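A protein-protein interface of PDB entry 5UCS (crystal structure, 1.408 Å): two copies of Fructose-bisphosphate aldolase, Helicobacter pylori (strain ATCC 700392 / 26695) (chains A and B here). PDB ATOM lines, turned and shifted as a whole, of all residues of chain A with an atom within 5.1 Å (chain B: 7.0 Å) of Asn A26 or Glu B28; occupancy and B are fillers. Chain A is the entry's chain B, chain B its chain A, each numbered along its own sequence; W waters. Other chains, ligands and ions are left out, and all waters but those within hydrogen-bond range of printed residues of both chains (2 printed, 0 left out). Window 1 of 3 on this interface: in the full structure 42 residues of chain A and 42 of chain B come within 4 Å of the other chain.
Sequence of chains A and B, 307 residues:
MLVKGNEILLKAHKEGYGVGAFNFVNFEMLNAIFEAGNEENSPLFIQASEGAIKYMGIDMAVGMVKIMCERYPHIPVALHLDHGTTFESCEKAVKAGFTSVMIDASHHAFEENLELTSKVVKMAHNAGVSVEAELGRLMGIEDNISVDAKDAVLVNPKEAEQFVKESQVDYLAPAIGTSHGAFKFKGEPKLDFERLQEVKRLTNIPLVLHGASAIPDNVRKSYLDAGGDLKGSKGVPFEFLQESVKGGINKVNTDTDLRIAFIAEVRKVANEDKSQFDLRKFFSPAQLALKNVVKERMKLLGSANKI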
ATOM      1  N   PHE A  24     -15.483   7.573 -14.760  1.00  0.00           N
ATOM      2  CA  PHE A  24     -16.455   7.432 -13.692  1.00  0.00           C
ATOM      3  C   PHE A  24     -15.808   7.739 -12.353  1.00  0.00           C
ATOM      4  O   PHE A  24     -14.606   7.525 -12.175  1.00  0.00           O
ATOM      5  CB  PHE A  24     -17.106   6.040 -13.660  1.00  0.00           C
ATOM      6  CG  PHE A  24     -16.253   4.936 -13.098  1.00  0.00           C
ATOM      7  CD1 PHE A  24     -15.157   4.463 -13.764  1.00  0.00           C
ATOM      8  CD2 PHE A  24     -16.605   4.326 -11.902  1.00  0.00           C
ATOM      9  CE1 PHE A  24     -14.397   3.409 -13.247  1.00  0.00           C
ATOM     10  CE2 PHE A  24     -15.869   3.266 -11.392  1.00  0.00           C
ATOM     11  CZ  PHE A  24     -14.771   2.823 -12.046  1.00  0.00           C
ATOM     12  N   VAL A  25     -16.621   8.219 -11.405  1.00  0.00           N
ATOM     13  CA  VAL A  25     -16.191   8.386 -10.019  1.00  0.00           C
ATOM     14  C   VAL A  25     -17.073   7.647  -9.029  1.00  0.00           C
ATOM     15  O   VAL A  25     -16.767   7.640  -7.830  1.00  0.00           O
ATOM     16  CB  VAL A  25     -16.055   9.872  -9.596  1.00  0.00           C
ATOM     17  CG1 VAL A  25     -15.201  10.625 -10.559  1.00  0.00           C
ATOM     18  CG2 VAL A  25     -17.415  10.542  -9.437  1.00  0.00           C
ATOM     19  N   ASN A  26     -18.180   7.054  -9.456  1.00  0.00           N
ATOM     20  CA  ASN A  26     -19.067   6.372  -8.524  1.00  0.00           C
ATOM     21  C   ASN A  26     -20.023   5.460  -9.294  1.00  0.00           C
ATOM     22  O   ASN A  26     -19.882   5.249 -10.504  1.00  0.00           O
ATOM     23  CB  ASN A  26     -19.800   7.370  -7.633  1.00  0.00           C
ATOM     24  CG  ASN A  26     -20.827   8.228  -8.378  1.00  0.00           C
ATOM     25  OD1 ASN A  26     -21.169   7.992  -9.546  1.00  0.00           O
ATOM     26  ND2 ASN A  26     -21.368   9.221  -7.675  1.00  0.00           N
ATOM     27  N   PHE A  27     -20.971   4.870  -8.563  1.00  0.00           N
ATOM     28  CA  PHE A  27     -21.886   3.898  -9.149  1.00  0.00           C
ATOM     29  C   PHE A  27     -22.752   4.515 -10.239  1.00  0.00           C
ATOM     30  O   PHE A  27     -22.945   3.919 -11.305  1.00  0.00           O
ATOM     31  CB  PHE A  27     -22.769   3.255  -8.083  1.00  0.00           C
ATOM     32  CG  PHE A  27     -23.946   2.534  -8.678  1.00  0.00           C
ATOM     33  CD1 PHE A  27     -23.751   1.373  -9.398  1.00  0.00           C
ATOM     34  CD2 PHE A  27     -25.225   3.051  -8.585  1.00  0.00           C
ATOM     35  CE1 PHE A  27     -24.819   0.712  -9.997  1.00  0.00           C
ATOM     36  CE2 PHE A  27     -26.296   2.394  -9.206  1.00  0.00           C
ATOM     37  CZ  PHE A  27     -26.081   1.233  -9.897  1.00  0.00           C
ATOM     38  N   GLU A  28     -23.323   5.690  -9.988  1.00  0.00           N
ATOM     39  CA  GLU A  28     -24.279   6.253 -10.927  1.00  0.00           C
ATOM     40  C   GLU A  28     -23.640   6.488 -12.286  1.00  0.00           C
ATOM     41  O   GLU A  28     -24.243   6.187 -13.331  1.00  0.00           O
ATOM     42  CB  GLU A  28     -24.845   7.550 -10.371  1.00  0.00           C
ATOM     43  CG  GLU A  28     -25.959   7.335  -9.385  1.00  0.00           C
ATOM     44  CD  GLU A  28     -25.503   7.040  -7.973  1.00  0.00           C
ATOM     45  OE1 GLU A  28     -24.278   7.095  -7.664  1.00  0.00           O
ATOM     46  OE2 GLU A  28     -26.415   6.817  -7.143  1.00  0.00           O
ATOM     47  N   MET A  29     -22.431   7.061 -12.298  1.00  0.00           N
ATOM     48  CA  MET A  29     -21.761   7.285 -13.580  1.00  0.00           C
ATOM     49  C   MET A  29     -21.501   5.961 -14.273  1.00  0.00           C
ATOM     50  O   MET A  29     -21.685   5.832 -15.491  1.00  0.00           O
ATOM     51  CB  MET A  29     -20.451   8.035 -13.387  1.00  0.00           C
ATOM     52  CG  MET A  29     -20.573   9.455 -12.888  1.00  0.00           C
ATOM     53  SD  MET A  29     -19.027  10.375 -12.832  1.00  0.00           S
ATOM     54  CE  MET A  29     -18.780  10.815 -14.553  1.00  0.00           C
ATOM     55  N   LEU A  30     -21.020   4.975 -13.523  1.00  0.00           N
ATOM     56  CA  LEU A  30     -20.661   3.697 -14.129  1.00  0.00           C
ATOM     57  C   LEU A  30     -21.884   3.004 -14.712  1.00  0.00           C
ATOM     58  O   LEU A  30     -21.844   2.447 -15.820  1.00  0.00           O
ATOM     59  CB  LEU A  30     -19.981   2.808 -13.095  1.00  0.00           C
ATOM     60  CG  LEU A  30     -19.372   1.516 -13.621  1.00  0.00           C
ATOM     61  CD1 LEU A  30     -18.232   1.779 -14.566  1.00  0.00           C
ATOM     62  CD2 LEU A  30     -18.898   0.701 -12.414  1.00  0.00           C
ATOM     63  N   TYR A  55     -10.932   8.539  -4.330  1.00  0.00           N
ATOM     64  CA  TYR A  55     -12.298   8.769  -3.844  1.00  0.00           C
ATOM     65  C   TYR A  55     -13.026   7.450  -3.591  1.00  0.00           C
ATOM     66  O   TYR A  55     -13.619   7.238  -2.521  1.00  0.00           O
ATOM     67  CB  TYR A  55     -13.045   9.621  -4.872  1.00  0.00           C
ATOM     68  CG  TYR A  55     -14.503   9.909  -4.568  1.00  0.00           C
ATOM     69  CD1 TYR A  55     -14.850  10.948  -3.721  1.00  0.00           C
ATOM     70  CD2 TYR A  55     -15.529   9.159  -5.148  1.00  0.00           C
ATOM     71  CE1 TYR A  55     -16.159  11.233  -3.454  1.00  0.00           C
ATOM     72  CE2 TYR A  55     -16.847   9.442  -4.898  1.00  0.00           C
ATOM     73  CZ  TYR A  55     -17.166  10.472  -4.039  1.00  0.00           C
ATOM     74  OH  TYR A  55     -18.485  10.781  -3.730  1.00  0.00           O
ATOM     75  N   MET A  56     -12.972   6.537  -4.554  1.00  0.00           N
ATOM     76  CA  MET A  56     -13.660   5.264  -4.415  1.00  0.00           C
ATOM     77  C   MET A  56     -12.897   4.236  -3.585  1.00  0.00           C
ATOM     78  O   MET A  56     -13.528   3.351  -2.981  1.00  0.00           O
ATOM     79  CB  MET A  56     -13.877   4.660  -5.795  1.00  0.00           C
ATOM     80  CG  MET A  56     -15.041   5.263  -6.565  1.00  0.00           C
ATOM     81  SD  MET A  56     -15.282   4.526  -8.208  1.00  0.00           S
ATOM     82  CE  MET A  56     -13.962   5.334  -9.094  1.00  0.00           C
ATOM     83  N   MET A  64     -16.639  -2.656  -8.631  1.00  0.00           N
ATOM     84  CA  MET A  64     -17.888  -2.264  -9.273  1.00  0.00           C
ATOM     85  C   MET A  64     -17.829  -2.564 -10.762  1.00  0.00           C
ATOM     86  O   MET A  64     -18.834  -3.003 -11.348  1.00  0.00           O
ATOM     87  CB  MET A  64     -18.177  -0.776  -9.049  1.00  0.00           C
ATOM     88  CG  MET A  64     -18.651  -0.442  -7.631  1.00  0.00           C
ATOM     89  SD  MET A  64     -19.349   1.211  -7.500  1.00  0.00           S
ATOM     90  CE  MET A  64     -17.954   2.201  -7.980  1.00  0.00           C
ATOM     91  N   PHE B  24     -28.834   2.485   2.676  1.00  0.00           N
ATOM     92  CA  PHE B  24     -28.028   3.035   1.587  1.00  0.00           C
ATOM     93  C   PHE B  24     -28.707   2.823   0.243  1.00  0.00           C
ATOM     94  O   PHE B  24     -29.448   1.849   0.057  1.00  0.00           O
ATOM     95  CB  PHE B  24     -26.610   2.456   1.561  1.00  0.00           C
ATOM     96  CG  PHE B  24     -26.490   1.060   0.993  1.00  0.00           C
ATOM     97  CD1 PHE B  24     -26.983  -0.030   1.666  1.00  0.00           C
ATOM     98  CD2 PHE B  24     -25.841   0.849  -0.212  1.00  0.00           C
ATOM     99  CE1 PHE B  24     -26.836  -1.313   1.118  1.00  0.00           C
ATOM    100  CE2 PHE B  24     -25.670  -0.405  -0.715  1.00  0.00           C
ATOM    101  CZ  PHE B  24     -26.159  -1.476  -0.070  1.00  0.00           C
ATOM    102  N   VAL B  25     -28.418   3.732  -0.697  1.00  0.00           N
ATOM    103  CA  VAL B  25     -28.821   3.579  -2.094  1.00  0.00           C
ATOM    104  C   VAL B  25     -27.664   3.608  -3.071  1.00  0.00           C
ATOM    105  O   VAL B  25     -27.893   3.388  -4.267  1.00  0.00           O
ATOM    106  CB  VAL B  25     -29.906   4.579  -2.556  1.00  0.00           C
ATOM    107  CG1 VAL B  25     -31.103   4.524  -1.693  1.00  0.00           C
ATOM    108  CG2 VAL B  25     -29.365   5.982  -2.635  1.00  0.00           C
ATOM    109  N   ASN B  26     -26.446   3.904  -2.629  1.00  0.00           N
ATOM    110  CA  ASN B  26     -25.325   4.016  -3.545  1.00  0.00           C
ATOM    111  C   ASN B  26     -24.019   3.949  -2.764  1.00  0.00           C
ATOM    112  O   ASN B  26     -24.005   3.681  -1.558  1.00  0.00           O
ATOM    113  CB  ASN B  26     -25.445   5.264  -4.422  1.00  0.00           C
ATOM    114  CG  ASN B  26     -25.284   6.557  -3.666  1.00  0.00           C
ATOM    115  OD1 ASN B  26     -24.900   6.580  -2.489  1.00  0.00           O
ATOM    116  ND2 ASN B  26     -25.598   7.655  -4.334  1.00  0.00           N
ATOM    117  N   PHE B  27     -22.918   4.184  -3.463  1.00  0.00           N
ATOM    118  CA  PHE B  27     -21.591   4.058  -2.868  1.00  0.00           C
ATOM    119  C   PHE B  27     -21.363   5.115  -1.794  1.00  0.00           C
ATOM    120  O   PHE B  27     -20.825   4.819  -0.721  1.00  0.00           O
ATOM    121  CB  PHE B  27     -20.496   4.132  -3.947  1.00  0.00           C
ATOM    122  CG  PHE B  27     -19.146   4.398  -3.360  1.00  0.00           C
ATOM    123  CD1 PHE B  27     -18.486   3.403  -2.669  1.00  0.00           C
ATOM    124  CD2 PHE B  27     -18.588   5.651  -3.402  1.00  0.00           C
ATOM    125  CE1 PHE B  27     -17.255   3.638  -2.063  1.00  0.00           C
ATOM    126  CE2 PHE B  27     -17.341   5.908  -2.804  1.00  0.00           C
ATOM    127  CZ  PHE B  27     -16.681   4.893  -2.137  1.00  0.00           C
ATOM    128  N   GLU B  28     -21.761   6.359  -2.050  1.00  0.00           N
ATOM    129  CA  GLU B  28     -21.471   7.429  -1.100  1.00  0.00           C
ATOM    130  C   GLU B  28     -22.103   7.154   0.264  1.00  0.00           C
ATOM    131  O   GLU B  28     -21.467   7.324   1.316  1.00  0.00           O
ATOM    132  CB  GLU B  28     -21.973   8.752  -1.662  1.00  0.00           C
ATOM    133  CG  GLU B  28     -21.018   9.397  -2.673  1.00  0.00           C
ATOM    134  CD  GLU B  28     -21.068   8.809  -4.071  1.00  0.00           C
ATOM    135  OE1 GLU B  28     -21.989   7.998  -4.353  1.00  0.00           O
ATOM    136  OE2 GLU B  28     -20.213   9.214  -4.893  1.00  0.00           O
ATOM    137  N   MET B  29     -23.376   6.756   0.279  1.00  0.00           N
ATOM    138  CA  MET B  29     -24.017   6.466   1.562  1.00  0.00           C
ATOM    139  C   MET B  29     -23.317   5.314   2.258  1.00  0.00           C
ATOM    140  O   MET B  29     -23.022   5.380   3.463  1.00  0.00           O
ATOM    141  CB  MET B  29     -25.477   6.126   1.325  1.00  0.00           C
ATOM    142  CG  MET B  29     -26.318   7.261   0.780  1.00  0.00           C
ATOM    143  SD  MET B  29     -28.087   6.906   0.788  1.00  0.00           S
ATOM    144  CE  MET B  29     -28.540   7.053   2.516  1.00  0.00           C
ATOM    145  N   LEU B  30     -23.032   4.248   1.514  1.00  0.00           N
ATOM    146  CA  LEU B  30     -22.401   3.067   2.096  1.00  0.00           C
ATOM    147  C   LEU B  30     -21.029   3.385   2.690  1.00  0.00           C
ATOM    148  O   LEU B  30     -20.679   2.912   3.785  1.00  0.00           O
ATOM    149  CB  LEU B  30     -22.296   1.967   1.040  1.00  0.00           C
ATOM    150  CG  LEU B  30     -21.843   0.600   1.532  1.00  0.00           C
ATOM    151  CD1 LEU B  30     -22.813   0.018   2.535  1.00  0.00           C
ATOM    152  CD2 LEU B  30     -21.645  -0.328   0.352  1.00  0.00           C
ATOM    153  N   ASN B  31     -20.218   4.151   1.967  1.00  0.00           N
ATOM    154  CA  ASN B  31     -18.870   4.468   2.433  1.00  0.00           C
ATOM    155  C   ASN B  31     -18.937   5.262   3.728  1.00  0.00           C
ATOM    156  O   ASN B  31     -18.202   4.971   4.688  1.00  0.00           O
ATOM    157  CB  ASN B  31     -18.102   5.229   1.351  1.00  0.00           C
ATOM    158  CG  ASN B  31     -16.642   5.381   1.681  1.00  0.00           C
ATOM    159  OD1 ASN B  31     -15.973   4.414   2.059  1.00  0.00           O
ATOM    160  ND2 ASN B  31     -16.137   6.599   1.555  1.00  0.00           N
ATOM    161  N   ALA B  32     -19.828   6.249   3.781  1.00  0.00           N
ATOM    162  CA  ALA B  32     -19.979   7.068   4.978  1.00  0.00           C
ATOM    163  C   ALA B  32     -20.420   6.240   6.180  1.00  0.00           C
ATOM    164  O   ALA B  32     -19.942   6.462   7.300  1.00  0.00           O
ATOM    165  CB  ALA B  32     -20.949   8.214   4.692  1.00  0.00           C
ATOM    166  N   ILE B  33     -21.348   5.307   5.969  1.00  0.00           N
ATOM    167  CA  ILE B  33     -21.818   4.449   7.064  1.00  0.00           C
ATOM    168  C   ILE B  33     -20.669   3.600   7.602  1.00  0.00           C
ATOM    169  O   ILE B  33     -20.490   3.452   8.825  1.00  0.00           O
ATOM    170  CB  ILE B  33     -22.987   3.579   6.580  1.00  0.00           C
ATOM    171  CG1 ILE B  33     -24.211   4.443   6.302  1.00  0.00           C
ATOM    172  CG2 ILE B  33     -23.341   2.503   7.601  1.00  0.00           C
ATOM    173  CD1 ILE B  33     -25.253   3.731   5.460  1.00  0.00           C
ATOM    174  N   MET B  64     -21.101  -4.368  -3.449  1.00  0.00           N
ATOM    175  CA  MET B  64     -20.447  -3.243  -2.778  1.00  0.00           C
ATOM    176  C   MET B  64     -20.286  -3.500  -1.284  1.00  0.00           C
ATOM    177  O   MET B  64     -19.263  -3.137  -0.690  1.00  0.00           O
ATOM    178  CB  MET B  64     -21.188  -1.917  -3.009  1.00  0.00           C
ATOM    179  CG  MET B  64     -21.130  -1.389  -4.434  1.00  0.00           C
ATOM    180  SD  MET B  64     -21.736   0.304  -4.599  1.00  0.00           S
ATOM    181  CE  MET B  64     -23.359   0.178  -3.871  1.00  0.00           C
ATOM    182  N   PHE B 262     -27.147  14.576   3.898  1.00  0.00           N
ATOM    183  CA  PHE B 262     -26.401  14.416   2.653  1.00  0.00           C
ATOM    184  C   PHE B 262     -26.829  15.459   1.638  1.00  0.00           C
ATOM    185  O   PHE B 262     -25.997  16.174   1.073  1.00  0.00           O
ATOM    186  CB  PHE B 262     -26.674  13.008   2.113  1.00  0.00           C
ATOM    187  CG  PHE B 262     -25.844  12.610   0.920  1.00  0.00           C
ATOM    188  CD1 PHE B 262     -24.698  11.831   1.079  1.00  0.00           C
ATOM    189  CD2 PHE B 262     -26.223  12.969  -0.356  1.00  0.00           C
ATOM    190  CE1 PHE B 262     -23.943  11.456  -0.011  1.00  0.00           C
ATOM    191  CE2 PHE B 262     -25.470  12.572  -1.445  1.00  0.00           C
ATOM    192  CZ  PHE B 262     -24.333  11.841  -1.272  1.00  0.00           C
ATOM    193  N   LEU B 279     -18.234  15.891  -9.393  1.00  0.00           N
ATOM    194  CA  LEU B 279     -19.106  15.176  -8.460  1.00  0.00           C
ATOM    195  C   LEU B 279     -18.484  15.053  -7.087  1.00  0.00           C
ATOM    196  O   LEU B 279     -19.220  15.033  -6.086  1.00  0.00           O
ATOM    197  CB  LEU B 279     -19.480  13.792  -8.986  1.00  0.00           C
ATOM    198  CG  LEU B 279     -20.653  13.722  -9.975  1.00  0.00           C
ATOM    199  CD1 LEU B 279     -20.365  14.508 -11.251  1.00  0.00           C
ATOM    200  CD2 LEU B 279     -20.953  12.254 -10.285  1.00  0.00           C
ATOM    201  N   ARG B 280     -17.160  14.935  -7.000  1.00  0.00           N
ATOM    202  CA  ARG B 280     -16.525  14.788  -5.692  1.00  0.00           C
ATOM    203  C   ARG B 280     -16.710  16.026  -4.833  1.00  0.00           C
ATOM    204  O   ARG B 280     -16.778  15.932  -3.599  1.00  0.00           O
ATOM    205  CB  ARG B 280     -15.045  14.483  -5.854  1.00  0.00           C
ATOM    206  CG  ARG B 280     -14.727  13.200  -6.588  1.00  0.00           C
ATOM    207  CD  ARG B 280     -13.209  13.104  -6.838  1.00  0.00           C
ATOM    208  NE  ARG B 280     -12.716  14.273  -7.573  1.00  0.00           N
ATOM    209  CZ  ARG B 280     -11.434  14.582  -7.743  1.00  0.00           C
ATOM    210  NH1 ARG B 280     -11.093  15.670  -8.427  1.00  0.00           N
ATOM    211  NH2 ARG B 280     -10.489  13.818  -7.223  1.00  0.00           N
ATOM    212  N   PHE B 283     -20.084  15.504  -3.332  1.00  0.00           N
ATOM    213  CA  PHE B 283     -20.380  14.309  -2.554  1.00  0.00           C
ATOM    214  C   PHE B 283     -19.398  14.033  -1.423  1.00  0.00           C
ATOM    215  O   PHE B 283     -19.756  13.290  -0.494  1.00  0.00           O
ATOM    216  CB  PHE B 283     -20.553  13.090  -3.460  1.00  0.00           C
ATOM    217  CG  PHE B 283     -21.640  13.243  -4.482  1.00  0.00           C
ATOM    218  CD1 PHE B 283     -22.767  14.024  -4.251  1.00  0.00           C
ATOM    219  CD2 PHE B 283     -21.511  12.622  -5.701  1.00  0.00           C
ATOM    220  CE1 PHE B 283     -23.753  14.151  -5.222  1.00  0.00           C
ATOM    221  CE2 PHE B 283     -22.484  12.734  -6.665  1.00  0.00           C
ATOM    222  CZ  PHE B 283     -23.596  13.516  -6.446  1.00  0.00           C
ATOM    223  N   SER B 284     -18.193  14.615  -1.452  1.00  0.00           N
ATOM    224  CA  SER B 284     -17.312  14.496  -0.294  1.00  0.00           C
ATOM    225  C   SER B 284     -17.893  15.197   0.922  1.00  0.00           C
ATOM    226  O   SER B 284     -17.992  14.555   1.985  1.00  0.00           O
ATOM    227  CB  SER B 284     -15.890  14.941  -0.631  1.00  0.00           C
ATOM    228  OG  SER B 284     -15.308  13.990  -1.515  1.00  0.00           O
ATOM    229  N   ALA B 286     -21.023  15.874   1.411  1.00  0.00           N
ATOM    230  CA  ALA B 286     -22.254  15.156   1.703  1.00  0.00           C
ATOM    231  C   ALA B 286     -21.971  13.867   2.467  1.00  0.00           C
ATOM    232  O   ALA B 286     -22.665  13.547   3.438  1.00  0.00           O
ATOM    233  CB  ALA B 286     -22.972  14.870   0.388  1.00  0.00           C
ATOM    234  N   GLN B 287     -20.927  13.136   2.071  1.00  0.00           N
ATOM    235  CA  GLN B 287     -20.538  11.947   2.821  1.00  0.00           C
ATOM    236  C   GLN B 287     -20.178  12.307   4.252  1.00  0.00           C
ATOM    237  O   GLN B 287     -20.529  11.590   5.181  1.00  0.00           O
ATOM    238  CB  GLN B 287     -19.333  11.257   2.191  1.00  0.00           C
ATOM    239  CG  GLN B 287     -19.612  10.416   0.976  1.00  0.00           C
ATOM    240  CD  GLN B 287     -18.393   9.622   0.583  1.00  0.00           C
ATOM    241  OE1 GLN B 287     -17.865   8.846   1.380  1.00  0.00           O
ATOM    242  NE2 GLN B 287     -17.918   9.836  -0.648  1.00  0.00           N
ATOM    243  N   LEU B 290     -23.258  12.933   6.347  1.00  0.00           N
ATOM    244  CA  LEU B 290     -23.966  11.691   6.625  1.00  0.00           C
ATOM    245  C   LEU B 290     -23.197  10.871   7.645  1.00  0.00           C
ATOM    246  O   LEU B 290     -23.776  10.367   8.625  1.00  0.00           O
ATOM    247  CB  LEU B 290     -24.162  10.924   5.314  1.00  0.00           C
ATOM    248  CG  LEU B 290     -25.081   9.718   5.364  1.00  0.00           C
ATOM    249  CD1 LEU B 290     -25.663   9.450   3.971  1.00  0.00           C
ATOM    250  CD2 LEU B 290     -24.395   8.470   5.896  1.00  0.00           C
HETATM  251  O   HOH W   1     -15.070   8.930  -0.772  1.00  0.00           O
HETATM  252  O   HOH W   2     -22.519   5.987  -6.034  1.00  0.00           O
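The side-chain hydroxyl (OG) of Ser B284 sits at hydrogen-bond distance from the backbone carbonyl oxygen (O) of Arg B280, 3.2 Å away. OD1 of Asn A26 is in hydrogen-bond range of N of Glu A28, 3.2 Å away. The side-chain amide oxygen (OE1) of Gln B287 is in hydrogen-bond range of the side-chain amide nitrogen (ND2) of Asn B31 (2.8 Å). The side-chain sulfur of Met A29 is in hydrogen-bond range of the backbone NH of Val A25, at 3.5 Å. The side-chain amide oxygen (OD1) of Asn B26 is in hydrogen-bond range of the backbone NH (N) of Met B29 (3.2 Å). The backbone NH (N) of Met A29 lies within hydrogen-bond range of the side-chain amide oxygen (OD1) of Asn A26, 3.2 Å away.
Water W2 lies within hydrogen-bond range of OE1 of Glu A28 (2.6 Å), OE1 of Glu B28 (2.7 Å), N of Phe B27 (3.2 Å) and N of Phe A27 (3.2 Å). Water W1 lies within hydrogen-bond range of O of Tyr A55, NE2 of Gln B287 and ND2 of Asn B31.
Phe A24 touches none of the printed residues of chain B. Of the printed residues of chain B, Val A25 touches Leu B279. Asn A26 touches two residues of chain B. Of the printed residues of chain A, Phe B27 touches Tyr A55 and Met A56. Of the printed residues of chain A, Met B64 touches Met A64 (3.9 Å). The nearest residue of chain B that does not touch Asn A26 is Leu B279 (4.02 Å). The nearest residue of chain A that does not touch Glu B28 is Glu A28 (4.1 Å).
ND2 of Asn A26 is in hydrogen-bond range of OE2 of Glu B28 (3.0 Å). The side-chain amide nitrogen (NE2) of Gln B287 is in hydrogen-bond range of the side-chain hydroxyl (OH) of Tyr A55, at 3.3 Å. The side-chain carboxylate of Glu A28 sits at hydrogen-bond distance from the side-chain amide nitrogen of Asn B26, at 3.0 Å. OE2 of Glu B28 lies within hydrogen-bond range of OH of Tyr A55, at 2.6 Å.
CG2 of Val A25 touches CB of Leu B279, 3.9 Å away. Phe B283 touches Asn A26. SD of Met A29 touches CD2 of Leu B279 (3.7 Å). O of Tyr A55 touches CZ of Phe B27, 3.9 Å away. Tyr A55 touches Arg B280. CB of Phe B283 touches OH of Tyr A55 (3.1 Å). Tyr A55 touches Ser B284. Phe B27 touches Met A56 (CZ to O, 3.6 Å). Met B64 touches Met A64.
Asn A26 touches Glu B28, and with the chains exchanged Glu A28 touches Asn B26. Met A64 touches its own counterpart, Met B64. Positions printed for both chains: 24, 25, 26, 27, 28, 29, 30 and 64. Of the 13 pairs that touch across the chains among the printed residues, 3 have their exchanged pair printed and touching as well.
Of the 19 printed residues of chain B, 9 touch a printed residue of chain A. Hydrophobic or aromatic side chains of chain B within 4 Å of the printed part of chain A: Phe B27, Met B64, Leu B279 and Phe B283. Printed residues of chain A that touch a printed residue of chain B: Val A25, Asn A26, Glu A28, Met A29, Tyr A55, Met A56 and Met A64. Among the printed residues, no Asp or Glu carboxylate lies within 4 Å of a Lys or Arg side-chain nitrogen of the other chain.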
